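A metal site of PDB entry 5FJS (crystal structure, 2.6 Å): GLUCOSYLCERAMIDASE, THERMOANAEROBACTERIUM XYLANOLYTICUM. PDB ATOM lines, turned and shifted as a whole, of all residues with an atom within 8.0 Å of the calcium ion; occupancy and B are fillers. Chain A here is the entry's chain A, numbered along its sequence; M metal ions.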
ATOM      1  N   LYS A 553      15.381  -2.569   0.083  1.00  0.00           N
ATOM      2  CA  LYS A 553      16.483  -2.962  -0.804  1.00  0.00           C
ATOM      3  C   LYS A 553      16.252  -2.593  -2.270  1.00  0.00           C
ATOM      4  O   LYS A 553      17.197  -2.271  -2.961  1.00  0.00           O
ATOM      5  CB  LYS A 553      16.740  -4.448  -0.712  1.00  0.00           C
ATOM      6  CG  LYS A 553      17.890  -4.973  -1.558  1.00  0.00           C
ATOM      7  CD  LYS A 553      19.268  -4.479  -1.145  1.00  0.00           C
ATOM      8  CE  LYS A 553      20.326  -5.504  -1.533  1.00  0.00           C
ATOM      9  NZ  LYS A 553      21.402  -4.965  -2.387  1.00  0.00           N
ATOM     10  N   MET A 555      15.190  -0.016  -3.433  1.00  0.00           N
ATOM     11  CA  MET A 555      15.468   1.395  -3.624  1.00  0.00           C
ATOM     12  C   MET A 555      16.934   1.712  -3.572  1.00  0.00           C
ATOM     13  O   MET A 555      17.300   2.887  -3.512  1.00  0.00           O
ATOM     14  CB  MET A 555      14.729   2.197  -2.561  1.00  0.00           C
ATOM     15  CG  MET A 555      13.231   1.999  -2.629  1.00  0.00           C
ATOM     16  SD  MET A 555      12.426   2.733  -1.199  1.00  0.00           S
ATOM     17  CE  MET A 555      10.825   1.998  -1.473  1.00  0.00           C
ATOM     18  N   ASP A 556      17.788   0.690  -3.573  1.00  0.00           N
ATOM     19  CA  ASP A 556      19.225   0.849  -3.776  1.00  0.00           C
ATOM     20  C   ASP A 556      19.486   0.865  -5.284  1.00  0.00           C
ATOM     21  O   ASP A 556      19.920  -0.127  -5.875  1.00  0.00           O
ATOM     22  CB  ASP A 556      19.961  -0.285  -3.068  1.00  0.00           C
ATOM     23  CG  ASP A 556      21.463  -0.230  -3.259  1.00  0.00           C
ATOM     24  OD1 ASP A 556      22.041   0.829  -3.603  1.00  0.00           O
ATOM     25  OD2 ASP A 556      22.065  -1.292  -3.027  1.00  0.00           O
ATOM     26  N   LYS A 557      19.209   1.996  -5.912  1.00  0.00           N
ATOM     27  CA  LYS A 557      19.369   2.178  -7.350  1.00  0.00           C
ATOM     28  C   LYS A 557      20.845   2.417  -7.776  1.00  0.00           C
ATOM     29  O   LYS A 557      21.137   2.357  -8.972  1.00  0.00           O
ATOM     30  CB  LYS A 557      18.412   3.256  -7.871  1.00  0.00           C
ATOM     31  N   ASP A 558      21.754   2.662  -6.829  1.00  0.00           N
ATOM     32  CA  ASP A 558      23.201   2.796  -7.168  1.00  0.00           C
ATOM     33  C   ASP A 558      24.059   1.604  -6.780  1.00  0.00           C
ATOM     34  O   ASP A 558      25.287   1.714  -6.835  1.00  0.00           O
ATOM     35  CB  ASP A 558      23.819   4.101  -6.582  1.00  0.00           C
ATOM     36  CG  ASP A 558      23.799   4.184  -5.026  1.00  0.00           C
ATOM     37  OD1 ASP A 558      23.483   3.216  -4.304  1.00  0.00           O
ATOM     38  OD2 ASP A 558      24.110   5.274  -4.493  1.00  0.00           O
ATOM     39  N   ASN A 559      23.440   0.490  -6.364  1.00  0.00           N
ATOM     40  CA  ASN A 559      24.154  -0.759  -6.012  1.00  0.00           C
ATOM     41  C   ASN A 559      25.351  -0.657  -5.044  1.00  0.00           C
ATOM     42  O   ASN A 559      26.341  -1.346  -5.197  1.00  0.00           O
ATOM     43  CB  ASN A 559      24.595  -1.490  -7.290  1.00  0.00           C
ATOM     44  CG  ASN A 559      23.536  -1.447  -8.360  1.00  0.00           C
ATOM     45  OD1 ASN A 559      23.730  -0.838  -9.419  1.00  0.00           O
ATOM     46  ND2 ASN A 559      22.388  -2.050  -8.067  1.00  0.00           N
ATOM     47  N   ASP A 560      25.232   0.217  -4.050  1.00  0.00           N
ATOM     48  CA  ASP A 560      26.166   0.265  -2.933  1.00  0.00           C
ATOM     49  C   ASP A 560      25.596  -0.453  -1.730  1.00  0.00           C
ATOM     50  O   ASP A 560      26.147  -0.344  -0.669  1.00  0.00           O
ATOM     51  CB  ASP A 560      26.517   1.704  -2.564  1.00  0.00           C
ATOM     52  CG  ASP A 560      25.388   2.393  -1.822  1.00  0.00           C
ATOM     53  OD1 ASP A 560      24.276   1.789  -1.755  1.00  0.00           O
ATOM     54  OD2 ASP A 560      25.613   3.534  -1.327  1.00  0.00           O
ATOM     55  N   GLY A 561      24.487  -1.176  -1.874  1.00  0.00           N
ATOM     56  CA  GLY A 561      23.917  -1.939  -0.770  1.00  0.00           C
ATOM     57  C   GLY A 561      22.949  -1.238   0.162  1.00  0.00           C
ATOM     58  O   GLY A 561      22.309  -1.901   0.971  1.00  0.00           O
ATOM     59  N   ILE A 562      22.819   0.085   0.021  1.00  0.00           N
ATOM     60  CA  ILE A 562      22.058   0.922   0.930  1.00  0.00           C
ATOM     61  C   ILE A 562      20.929   1.579   0.136  1.00  0.00           C
ATOM     62  O   ILE A 562      21.145   1.998  -0.992  1.00  0.00           O
ATOM     63  CB  ILE A 562      22.981   1.983   1.549  1.00  0.00           C
ATOM     64  CG1 ILE A 562      24.257   1.315   2.036  1.00  0.00           C
ATOM     65  CG2 ILE A 562      22.275   2.724   2.683  1.00  0.00           C
ATOM     66  CD1 ILE A 562      25.179   2.208   2.838  1.00  0.00           C
ATOM     67  N   PRO A 563      19.713   1.672   0.706  1.00  0.00           N
ATOM     68  CA  PRO A 563      18.658   2.387  -0.011  1.00  0.00           C
ATOM     69  C   PRO A 563      19.034   3.853  -0.288  1.00  0.00           C
ATOM     70  O   PRO A 563      19.734   4.463   0.520  1.00  0.00           O
ATOM     71  CB  PRO A 563      17.443   2.282   0.926  1.00  0.00           C
ATOM     72  CG  PRO A 563      17.969   1.817   2.225  1.00  0.00           C
ATOM     73  CD  PRO A 563      19.217   1.075   1.955  1.00  0.00           C
ATOM     74  N   ASP A 564      18.599   4.393  -1.440  1.00  0.00           N
ATOM     75  CA  ASP A 564      19.031   5.731  -1.942  1.00  0.00           C
ATOM     76  C   ASP A 564      18.069   6.830  -1.507  1.00  0.00           C
ATOM     77  O   ASP A 564      16.916   6.816  -1.922  1.00  0.00           O
ATOM     78  CB  ASP A 564      19.028   5.780  -3.485  1.00  0.00           C
ATOM     79  CG  ASP A 564      20.049   4.863  -4.162  1.00  0.00           C
ATOM     80  OD1 ASP A 564      20.665   3.984  -3.494  1.00  0.00           O
ATOM     81  OD2 ASP A 564      20.211   5.015  -5.415  1.00  0.00           O
ATOM     82  N   ASN A 565      18.517   7.786  -0.710  1.00  0.00           N
ATOM     83  CA  ASN A 565      17.701   8.979  -0.481  1.00  0.00           C
ATOM     84  C   ASN A 565      17.684   9.777  -1.792  1.00  0.00           C
ATOM     85  O   ASN A 565      18.667   9.853  -2.495  1.00  0.00           O
ATOM     86  CB  ASN A 565      18.236   9.785   0.689  1.00  0.00           C
ATOM     87  CG  ASN A 565      17.871   9.175   2.045  1.00  0.00           C
ATOM     88  OD1 ASN A 565      18.694   8.689   2.794  1.00  0.00           O
ATOM     89  ND2 ASN A 565      16.601   9.206   2.363  1.00  0.00           N
ATOM     90  N   GLY A 580      21.374  10.731  -1.814  1.00  0.00           N
ATOM     91  CA  GLY A 580      22.461   9.763  -1.830  1.00  0.00           C
ATOM     92  C   GLY A 580      22.282   8.754  -0.699  1.00  0.00           C
ATOM     93  O   GLY A 580      21.193   8.285  -0.496  1.00  0.00           O
ATOM     94  N   THR A 581      23.356   8.445   0.007  1.00  0.00           N
ATOM     95  CA  THR A 581      23.334   7.672   1.227  1.00  0.00           C
ATOM     96  C   THR A 581      23.471   8.617   2.393  1.00  0.00           C
ATOM     97  O   THR A 581      24.349   9.477   2.370  1.00  0.00           O
ATOM     98  CB  THR A 581      24.536   6.745   1.313  1.00  0.00           C
ATOM     99  OG1 THR A 581      24.550   5.847   0.212  1.00  0.00           O
ATOM    100  CG2 THR A 581      24.526   5.966   2.593  1.00  0.00           C
ATOM    101  N   SER A 582      22.626   8.425   3.392  1.00  0.00           N
ATOM    102  CA  SER A 582      22.544   9.302   4.545  1.00  0.00           C
ATOM    103  C   SER A 582      23.003   8.545   5.780  1.00  0.00           C
ATOM    104  O   SER A 582      22.834   7.325   5.849  1.00  0.00           O
ATOM    105  CB  SER A 582      21.119   9.819   4.725  1.00  0.00           C
ATOM    106  OG  SER A 582      20.164   8.807   5.020  1.00  0.00           O
ATOM    107  N   TRP A 589      19.394   1.389   8.482  1.00  0.00           N
ATOM    108  CA  TRP A 589      19.307   0.237   7.607  1.00  0.00           C
ATOM    109  C   TRP A 589      20.269  -0.882   8.059  1.00  0.00           C
ATOM    110  O   TRP A 589      19.885  -2.068   8.061  1.00  0.00           O
ATOM    111  CB  TRP A 589      19.566   0.689   6.164  1.00  0.00           C
ATOM    112  CG  TRP A 589      19.900  -0.363   5.113  1.00  0.00           C
ATOM    113  CD1 TRP A 589      21.114  -0.537   4.487  1.00  0.00           C
ATOM    114  CD2 TRP A 589      19.019  -1.302   4.521  1.00  0.00           C
ATOM    115  NE1 TRP A 589      21.039  -1.529   3.577  1.00  0.00           N
ATOM    116  CE2 TRP A 589      19.760  -2.030   3.580  1.00  0.00           C
ATOM    117  CE3 TRP A 589      17.676  -1.621   4.710  1.00  0.00           C
ATOM    118  CZ2 TRP A 589      19.203  -3.068   2.830  1.00  0.00           C
ATOM    119  CZ3 TRP A 589      17.119  -2.659   3.960  1.00  0.00           C
ATOM    120  CH2 TRP A 589      17.875  -3.348   3.025  1.00  0.00           C
ATOM    121  N   ASN A 622      30.511   0.170   2.527  1.00  0.00           N
ATOM    122  CA  ASN A 622      30.252   1.383   1.794  1.00  0.00           C
ATOM    123  C   ASN A 622      29.754   2.536   2.625  1.00  0.00           C
ATOM    124  O   ASN A 622      29.990   3.684   2.250  1.00  0.00           O
ATOM    125  CB  ASN A 622      29.261   1.133   0.676  1.00  0.00           C
ATOM    126  CG  ASN A 622      29.839   0.264  -0.414  1.00  0.00           C
ATOM    127  OD1 ASN A 622      31.025   0.364  -0.769  1.00  0.00           O
ATOM    128  ND2 ASN A 622      28.997  -0.597  -0.978  1.00  0.00           N
ATOM    129  N   GLU A 626      31.703   5.898   2.377  1.00  0.00           N
ATOM    130  CA  GLU A 626      31.003   7.068   1.863  1.00  0.00           C
ATOM    131  C   GLU A 626      30.931   8.184   2.863  1.00  0.00           C
ATOM    132  O   GLU A 626      30.990   9.305   2.447  1.00  0.00           O
ATOM    133  CB  GLU A 626      29.584   6.733   1.384  1.00  0.00           C
ATOM    134  CG  GLU A 626      29.531   5.915   0.107  1.00  0.00           C
ATOM    135  CD  GLU A 626      28.197   5.146  -0.124  1.00  0.00           C
ATOM    136  OE1 GLU A 626      27.123   5.492   0.420  1.00  0.00           O
ATOM    137  OE2 GLU A 626      28.209   4.154  -0.876  1.00  0.00           O
ATOM    138  N   THR A 637      25.642  12.120   1.095  1.00  0.00           N
ATOM    139  CA  THR A 637      26.690  12.183   0.079  1.00  0.00           C
ATOM    140  C   THR A 637      26.421  13.160  -1.061  1.00  0.00           C
ATOM    141  O   THR A 637      27.351  13.496  -1.777  1.00  0.00           O
ATOM    142  CB  THR A 637      26.978  10.794  -0.565  1.00  0.00           C
ATOM    143  OG1 THR A 637      25.791  10.237  -1.197  1.00  0.00           O
ATOM    144  CG2 THR A 637      27.485   9.874   0.480  1.00  0.00           C
ATOM    145  N   GLU A 638      25.178  13.609  -1.249  1.00  0.00           N
ATOM    146  CA  GLU A 638      24.855  14.418  -2.434  1.00  0.00           C
ATOM    147  C   GLU A 638      24.123  15.747  -2.218  1.00  0.00           C
ATOM    148  O   GLU A 638      23.994  16.518  -3.150  1.00  0.00           O
ATOM    149  CB  GLU A 638      24.086  13.560  -3.424  1.00  0.00           C
ATOM    150  CG  GLU A 638      24.933  12.455  -4.071  1.00  0.00           C
ATOM    151  CD  GLU A 638      24.103  11.434  -4.851  1.00  0.00           C
ATOM    152  OE1 GLU A 638      22.937  11.722  -5.199  1.00  0.00           O
ATOM    153  OE2 GLU A 638      24.618  10.328  -5.075  1.00  0.00           O
HETATM  154 CA    CA M   1      22.346   3.196  -2.490  1.00  0.00          CA
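The backbone NH of Lys 557 is in hydrogen-bond range of the side-chain carboxylate of Asp 564 (3.2 Å).
The backbone NH (N) of Asp 564 lies within hydrogen-bond range of the backbone carbonyl oxygen (O) of Met 555 (2.9 Å).
The backbone NH (N) of Gly 561 lies within hydrogen-bond range of the side-chain carboxylate (OD2) of Asp 556 (2.7 Å).
The side-chain carboxylate (OD2) of Asp 560 sits at hydrogen-bond distance from the side-chain hydroxyl (OG1) of Thr 581, at 3.0 Å.
The side-chain carboxylate (OE2) of Glu 626 lies close to the side-chain carboxylate (OD2) of Asp 560, at 2.7 Å.
The side-chain carboxylate of Asp 556 lies within salt-bridge range of the side-chain amino group of Lys 553, at 3.8 Å.
The side-chain amide nitrogen (ND2) of Asn 622 is in hydrogen-bond range of the backbone carbonyl oxygen (O) of Asp 560, at 2.9 Å.
The side-chain carboxylate (OD1) of Asp 556 sits close to the backbone NH (N) of Asn 559 (3.1 Å).
The calcium ion is bound by OD1 of Asp 564, at 2.1 Å.
The calcium ion is bound by the side-chain carboxylate (OD1) of Asp 558 (2.1 Å).
The calcium ion is bound by the backbone carbonyl oxygen (O) of Ile 562, at 2.3 Å.
The side-chain carboxylate (OD1) of Asp 560 is bound to the calcium ion, at 2.5 Å.
The calcium ion is bound by OD1 of Asp 556, 2.6 Å away.
Five residues have an atom within 4 Å of the calcium ion: Asp 556, Asp 558, Asp 560, Ile 562 and Asp 564.
The nearest printed residue that does not touch the calcium ion is Pro 563 (4.03 Å).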
